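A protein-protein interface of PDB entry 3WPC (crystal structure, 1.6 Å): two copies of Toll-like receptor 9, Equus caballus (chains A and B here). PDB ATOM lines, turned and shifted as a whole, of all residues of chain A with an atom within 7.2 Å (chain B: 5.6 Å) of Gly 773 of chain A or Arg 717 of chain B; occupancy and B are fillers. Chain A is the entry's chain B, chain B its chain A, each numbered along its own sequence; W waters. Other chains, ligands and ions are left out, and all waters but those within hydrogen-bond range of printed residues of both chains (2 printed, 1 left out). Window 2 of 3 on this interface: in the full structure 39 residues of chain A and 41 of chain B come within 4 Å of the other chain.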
ATOM      1  N   ARG A 717      14.882  28.330  12.684  1.00  0.00           N
ATOM      2  CA  ARG A 717      14.555  27.742  11.373  1.00  0.00           C
ATOM      3  C   ARG A 717      15.798  27.526  10.493  1.00  0.00           C
ATOM      4  O   ARG A 717      15.709  27.017   9.388  1.00  0.00           O
ATOM      5  CB  ARG A 717      13.443  28.504  10.675  1.00  0.00           C
ATOM      6  CG  ARG A 717      12.126  28.525  11.468  1.00  0.00           C
ATOM      7  CD  ARG A 717      11.053  29.276  10.743  1.00  0.00           C
ATOM      8  NE  ARG A 717      10.654  28.547   9.539  1.00  0.00           N
ATOM      9  CZ  ARG A 717      10.489  29.045   8.327  1.00  0.00           C
ATOM     10  NH1 ARG A 717      10.619  30.316   8.063  1.00  0.00           N
ATOM     11  NH2 ARG A 717      10.067  28.234   7.358  1.00  0.00           N
ATOM     12  N   HIS A 742      14.047  24.728   8.627  1.00  0.00           N
ATOM     13  CA  HIS A 742      13.388  24.832   7.337  1.00  0.00           C
ATOM     14  C   HIS A 742      14.163  24.053   6.307  1.00  0.00           C
ATOM     15  O   HIS A 742      15.269  24.443   5.948  1.00  0.00           O
ATOM     16  CB  HIS A 742      13.193  26.304   6.945  1.00  0.00           C
ATOM     17  CG  HIS A 742      12.450  26.472   5.656  1.00  0.00           C
ATOM     18  ND1 HIS A 742      11.216  25.897   5.426  1.00  0.00           N
ATOM     19  CD2 HIS A 742      12.773  27.138   4.520  1.00  0.00           C
ATOM     20  CE1 HIS A 742      10.811  26.211   4.208  1.00  0.00           C
ATOM     21  NE2 HIS A 742      11.744  26.956   3.636  1.00  0.00           N
ATOM     22  N   GLY A 770      11.091  21.455  10.679  1.00  0.00           N
ATOM     23  CA  GLY A 770       9.825  22.073  10.988  1.00  0.00           C
ATOM     24  C   GLY A 770       8.914  22.333   9.799  1.00  0.00           C
ATOM     25  O   GLY A 770       7.689  22.646   9.964  1.00  0.00           O
ATOM     26  N   SER A 771       9.469  22.253   8.607  1.00  0.00           N
ATOM     27  CA  SER A 771       8.854  22.762   7.372  1.00  0.00           C
ATOM     28  C   SER A 771       9.824  22.406   6.235  1.00  0.00           C
ATOM     29  O   SER A 771      10.982  22.083   6.489  1.00  0.00           O
ATOM     30  CB  SER A 771       8.616  24.285   7.420  1.00  0.00           C
ATOM     31  OG  SER A 771       9.864  24.982   7.595  1.00  0.00           O
ATOM     32  N   PRO A 772       9.362  22.454   4.970  1.00  0.00           N
ATOM     33  CA  PRO A 772       8.001  22.654   4.480  1.00  0.00           C
ATOM     34  C   PRO A 772       7.195  21.358   4.428  1.00  0.00           C
ATOM     35  O   PRO A 772       7.752  20.241   4.433  1.00  0.00           O
ATOM     36  CB  PRO A 772       8.239  23.168   3.047  1.00  0.00           C
ATOM     37  CG  PRO A 772       9.469  22.443   2.620  1.00  0.00           C
ATOM     38  CD  PRO A 772      10.307  22.195   3.862  1.00  0.00           C
ATOM     39  N   GLY A 773       5.874  21.539   4.360  1.00  0.00           N
ATOM     40  CA  GLY A 773       4.955  20.483   3.983  1.00  0.00           C
ATOM     41  C   GLY A 773       5.200  19.221   4.791  1.00  0.00           C
ATOM     42  O   GLY A 773       5.358  19.264   6.032  1.00  0.00           O
ATOM     43  N   GLN A 774       5.288  18.091   4.097  1.00  0.00           N
ATOM     44  CA  GLN A 774       5.368  16.809   4.756  1.00  0.00           C
ATOM     45  C   GLN A 774       6.706  16.519   5.405  1.00  0.00           C
ATOM     46  O   GLN A 774       6.850  15.469   6.040  1.00  0.00           O
ATOM     47  CB  GLN A 774       5.071  15.677   3.765  1.00  0.00           C
ATOM     48  CG  GLN A 774       3.645  15.668   3.263  1.00  0.00           C
ATOM     49  CD  GLN A 774       2.695  15.015   4.244  1.00  0.00           C
ATOM     50  OE1 GLN A 774       2.297  15.626   5.233  1.00  0.00           O
ATOM     51  NE2 GLN A 774       2.323  13.765   3.976  1.00  0.00           N
ATOM     52  N   LEU A 775       7.695  17.405   5.244  1.00  0.00           N
ATOM     53  CA  LEU A 775       8.994  17.175   5.869  1.00  0.00           C
ATOM     54  C   LEU A 775       8.920  17.475   7.361  1.00  0.00           C
ATOM     55  O   LEU A 775       9.783  17.030   8.120  1.00  0.00           O
ATOM     56  CB  LEU A 775      10.149  17.967   5.207  1.00  0.00           C
ATOM     57  CG  LEU A 775      10.638  17.447   3.850  1.00  0.00           C
ATOM     58  CD1 LEU A 775       9.522  17.302   2.844  1.00  0.00           C
ATOM     59  CD2 LEU A 775      11.718  18.372   3.285  1.00  0.00           C
ATOM     60  N   GLN A 776       7.902  18.246   7.773  1.00  0.00           N
ATOM     61  CA  GLN A 776       7.758  18.591   9.189  1.00  0.00           C
ATOM     62  C   GLN A 776       7.707  17.314  10.079  1.00  0.00           C
ATOM     63  O   GLN A 776       6.923  16.410   9.807  1.00  0.00           O
ATOM     64  CB  GLN A 776       6.532  19.464   9.412  1.00  0.00           C
ATOM     65  CG  GLN A 776       6.366  19.818  10.871  1.00  0.00           C
ATOM     66  CD  GLN A 776       5.155  20.704  11.155  1.00  0.00           C
ATOM     67  OE1 GLN A 776       4.317  20.969  10.271  1.00  0.00           O
ATOM     68  NE2 GLN A 776       5.075  21.173  12.373  1.00  0.00           N
ATOM     69  N   GLY A 777       8.585  17.237  11.082  1.00  0.00           N
ATOM     70  CA  GLY A 777       8.730  16.133  12.002  1.00  0.00           C
ATOM     71  C   GLY A 777       9.648  15.003  11.561  1.00  0.00           C
ATOM     72  O   GLY A 777       9.890  14.067  12.331  1.00  0.00           O
ATOM     73  N   ARG A 778      10.182  15.136  10.365  1.00  0.00           N
ATOM     74  CA  ARG A 778      11.148  14.182   9.832  1.00  0.00           C
ATOM     75  C   ARG A 778      12.547  14.643  10.038  1.00  0.00           C
ATOM     76  O   ARG A 778      12.834  15.850  10.087  1.00  0.00           O
ATOM     77  CB  ARG A 778      10.887  13.942   8.345  1.00  0.00           C
ATOM     78  CG  ARG A 778       9.974  12.742   8.122  1.00  0.00           C
ATOM     79  CD  ARG A 778       8.728  13.062   7.342  1.00  0.00           C
ATOM     80  NE  ARG A 778       8.892  12.911   5.908  1.00  0.00           N
ATOM     81  CZ  ARG A 778       7.891  12.711   5.042  1.00  0.00           C
ATOM     82  NH1 ARG A 778       6.627  12.605   5.452  1.00  0.00           N
ATOM     83  NH2 ARG A 778       8.161  12.600   3.749  1.00  0.00           N
ATOM     84  N   ILE B 693       1.260  18.188  14.936  1.00  0.00           N
ATOM     85  CA  ILE B 693       1.597  18.837  13.679  1.00  0.00           C
ATOM     86  C   ILE B 693       0.537  18.702  12.635  1.00  0.00           C
ATOM     87  O   ILE B 693       0.599  19.369  11.601  1.00  0.00           O
ATOM     88  CB  ILE B 693       2.919  18.311  13.088  1.00  0.00           C
ATOM     89  CG1 ILE B 693       2.753  16.902  12.507  1.00  0.00           C
ATOM     90  CG2 ILE B 693       4.011  18.380  14.136  1.00  0.00           C
ATOM     91  CD1 ILE B 693       3.949  16.423  11.714  1.00  0.00           C
ATOM     92  N   ALA B 715       2.396  22.327  17.350  1.00  0.00           N
ATOM     93  CA  ALA B 715       3.263  22.616  16.189  1.00  0.00           C
ATOM     94  C   ALA B 715       2.433  22.790  14.882  1.00  0.00           C
ATOM     95  O   ALA B 715       2.868  22.439  13.762  1.00  0.00           O
ATOM     96  CB  ALA B 715       4.269  21.498  16.053  1.00  0.00           C
ATOM     97  N   LEU B 716       1.202  23.298  15.025  1.00  0.00           N
ATOM     98  CA  LEU B 716       0.334  23.383  13.884  1.00  0.00           C
ATOM     99  C   LEU B 716       0.715  24.568  12.976  1.00  0.00           C
ATOM    100  O   LEU B 716       0.786  25.725  13.444  1.00  0.00           O
ATOM    101  CB  LEU B 716      -1.096  23.601  14.352  1.00  0.00           C
ATOM    102  CG  LEU B 716      -1.747  22.402  14.998  1.00  0.00           C
ATOM    103  CD1 LEU B 716      -3.014  22.874  15.715  1.00  0.00           C
ATOM    104  CD2 LEU B 716      -2.034  21.282  14.023  1.00  0.00           C
ATOM    105  N   ARG B 717       0.908  24.304  11.695  1.00  0.00           N
ATOM    106  CA  ARG B 717       1.247  25.335  10.756  1.00  0.00           C
ATOM    107  C   ARG B 717       0.053  25.885  10.000  1.00  0.00           C
ATOM    108  O   ARG B 717       0.193  26.781   9.177  1.00  0.00           O
ATOM    109  CB  ARG B 717       2.351  24.835   9.832  1.00  0.00           C
ATOM    110  CG  ARG B 717       3.609  24.450  10.568  1.00  0.00           C
ATOM    111  CD  ARG B 717       4.740  24.090   9.643  1.00  0.00           C
ATOM    112  NE  ARG B 717       5.173  25.260   8.866  1.00  0.00           N
ATOM    113  CZ  ARG B 717       5.386  25.296   7.568  1.00  0.00           C
ATOM    114  NH1 ARG B 717       5.253  24.216   6.808  1.00  0.00           N
ATOM    115  NH2 ARG B 717       5.839  26.440   7.052  1.00  0.00           N
ATOM    116  N   THR B 718      -1.107  25.294  10.258  1.00  0.00           N
ATOM    117  CA  THR B 718      -2.341  25.730   9.662  1.00  0.00           C
ATOM    118  C   THR B 718      -3.486  25.573  10.663  1.00  0.00           C
ATOM    119  O   THR B 718      -3.328  24.926  11.693  1.00  0.00           O
ATOM    120  CB  THR B 718      -2.612  24.924   8.377  1.00  0.00           C
ATOM    121  OG1 THR B 718      -3.646  25.584   7.654  1.00  0.00           O
ATOM    122  CG2 THR B 718      -2.955  23.513   8.630  1.00  0.00           C
ATOM    123  N   VAL B 719      -4.633  26.178  10.344  1.00  0.00           N
ATOM    124  CA  VAL B 719      -5.902  25.899  11.037  1.00  0.00           C
ATOM    125  C   VAL B 719      -6.974  25.653   9.948  1.00  0.00           C
ATOM    126  O   VAL B 719      -7.161  26.485   9.069  1.00  0.00           O
ATOM    127  CB  VAL B 719      -6.368  27.028  11.969  1.00  0.00           C
ATOM    128  CG1 VAL B 719      -7.523  26.519  12.805  1.00  0.00           C
ATOM    129  CG2 VAL B 719      -5.274  27.475  12.908  1.00  0.00           C
ATOM    130  N   PRO B 740       2.950  27.638  15.248  1.00  0.00           N
ATOM    131  CA  PRO B 740       3.801  28.207  14.193  1.00  0.00           C
ATOM    132  C   PRO B 740       3.080  28.302  12.841  1.00  0.00           C
ATOM    133  O   PRO B 740       3.434  27.665  11.845  1.00  0.00           O
ATOM    134  CB  PRO B 740       4.977  27.242  14.196  1.00  0.00           C
ATOM    135  CG  PRO B 740       4.329  25.957  14.508  1.00  0.00           C
ATOM    136  CD  PRO B 740       3.371  26.271  15.600  1.00  0.00           C
ATOM    137  N   LEU B 741       2.026  29.099  12.822  1.00  0.00           N
ATOM    138  CA  LEU B 741       1.224  29.252  11.655  1.00  0.00           C
ATOM    139  C   LEU B 741       2.029  29.771  10.481  1.00  0.00           C
ATOM    140  O   LEU B 741       2.880  30.657  10.605  1.00  0.00           O
ATOM    141  CB  LEU B 741      -0.013  30.091  11.926  1.00  0.00           C
ATOM    142  CG  LEU B 741      -0.912  29.629  13.046  1.00  0.00           C
ATOM    143  CD1 LEU B 741      -2.095  30.569  13.201  1.00  0.00           C
ATOM    144  CD2 LEU B 741      -1.457  28.250  12.737  1.00  0.00           C
ATOM    145  N   HIS B 742       1.800  29.136   9.321  1.00  0.00           N
ATOM    146  CA  HIS B 742       2.502  29.541   8.128  1.00  0.00           C
ATOM    147  C   HIS B 742       1.732  30.649   7.443  1.00  0.00           C
ATOM    148  O   HIS B 742       0.632  30.429   6.949  1.00  0.00           O
ATOM    149  CB  HIS B 742       2.754  28.359   7.230  1.00  0.00           C
ATOM    150  CG  HIS B 742       3.513  28.707   6.006  1.00  0.00           C
ATOM    151  ND1 HIS B 742       4.740  29.343   6.040  1.00  0.00           N
ATOM    152  CD2 HIS B 742       3.213  28.528   4.698  1.00  0.00           C
ATOM    153  CE1 HIS B 742       5.160  29.532   4.803  1.00  0.00           C
ATOM    154  NE2 HIS B 742       4.244  29.062   3.973  1.00  0.00           N
ATOM    155  N   PHE B 749      -6.301  29.389   7.200  1.00  0.00           N
ATOM    156  CA  PHE B 749      -6.598  29.812   8.512  1.00  0.00           C
ATOM    157  C   PHE B 749      -7.094  31.248   8.517  1.00  0.00           C
ATOM    158  O   PHE B 749      -7.882  31.582   9.346  1.00  0.00           O
ATOM    159  CB  PHE B 749      -5.396  29.582   9.433  1.00  0.00           C
ATOM    160  CG  PHE B 749      -4.318  30.620   9.338  1.00  0.00           C
ATOM    161  CD1 PHE B 749      -4.491  31.832   9.935  1.00  0.00           C
ATOM    162  CD2 PHE B 749      -3.105  30.349   8.714  1.00  0.00           C
ATOM    163  CE1 PHE B 749      -3.514  32.803   9.855  1.00  0.00           C
ATOM    164  CE2 PHE B 749      -2.086  31.313   8.701  1.00  0.00           C
ATOM    165  CZ  PHE B 749      -2.317  32.538   9.239  1.00  0.00           C
ATOM    166  N   SER B 771       6.380  31.430  10.371  1.00  0.00           N
ATOM    167  CA  SER B 771       6.981  31.457   9.039  1.00  0.00           C
ATOM    168  C   SER B 771       6.015  32.172   8.076  1.00  0.00           C
ATOM    169  O   SER B 771       4.871  32.444   8.439  1.00  0.00           O
ATOM    170  CB  SER B 771       7.240  30.034   8.537  1.00  0.00           C
ATOM    171  OG  SER B 771       5.988  29.319   8.367  1.00  0.00           O
HETATM  172  O   HOH W   1       4.857  24.289   3.998  1.00  0.00           O
HETATM  173  O   HOH W   2       4.490  21.539   7.535  1.00  0.00           O
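The backbone carbonyl oxygen (O) of Ala 715 of chain B sits at hydrogen-bond distance from the side-chain amide nitrogen (NE2) of Gln 776 of chain A (2.9 Å).
The guanidinium group (NH2) of Arg 717 of chain B lies within hydrogen-bond range of the side-chain hydroxyl (OG) of Ser 771 of chain B (3.2 Å).
A ring nitrogen (ND1) of His 742 of chain A is in hydrogen-bond range of the side-chain hydroxyl (OG) of Ser 771 of chain A (2.7 Å).
The backbone carbonyl oxygen (O) of Arg 717 of chain A lies within hydrogen-bond range of the backbone NH (N) of His 742 of chain A, 2.9 Å away.
NH2 of Arg 717 of chain A sits at hydrogen-bond distance from OG of Ser 771 of chain A, at 3.3 Å.
The backbone NH of His 742 of chain B lies within hydrogen-bond range of the backbone carbonyl oxygen of Arg 717 of chain B (2.9 Å).
A ring nitrogen (ND1) of His 742 of chain B sits at hydrogen-bond distance from the side-chain hydroxyl (OG) of Ser 771 of chain B.
Among the printed residues, pairs that only touch across the chains: Arg 717 of chain A with Ser 771 of chain B, Gly 770 of chain A with Arg 717 of chain B, Ser 771 of chain A with Arg 717 of chain B, Pro 772 of chain A with Arg 717 of chain B, Gly 773 of chain A with Arg 717 of chain B, Gln 776 of chain A with Ile 693 of chain B and Gln 776 of chain A with Arg 717 of chain B.
Of chain B, only Arg 717 comes within 4 Å of Gly 773 of chain A.
Arg 717 of chain B touches just these residues of chain A: Gly 770, Ser 771, Pro 772, Gly 773 and Gln 776.
Of the printed residues of chain A, Ala 715 of chain B touches Gln 776 (2.9 Å).
Of the printed residues of chain B, Gln 776 of chain A touches Ile 693, Ala 715 and Arg 717.
The nearest residue of chain A that does not touch Arg 717 of chain B is Arg 717 of chain A (4.6 Å).
The nearest printed residue of chain B that does not touch Arg 717 of chain A is Arg 717 of chain B (4.6 Å).
Hydrophobic or aromatic side chains of chain B within 4 Å of the printed part of chain A: Ile 693 and Ala 715.
Among the printed residues, 8 pairs touch across the chains.
Arg 717 of chain A touches Ser 771 of chain B, and with the chains exchanged Ser 771 of chain A touches Arg 717 of chain B.
3 positions are printed for both chains.
Water W2 lies within hydrogen-bond range of OE1 of Gln 776 of chain A (2.8 Å), O of Gly 773 of chain A (2.9 Å) and NH1 of Arg 717 of chain B (2.9 Å).
Water W1 bridges the guanidinium group (NH1) of Arg 717 of chain B (2.8 Å) and the backbone NH (N) of Gly 773 of chain A (3.0 Å).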
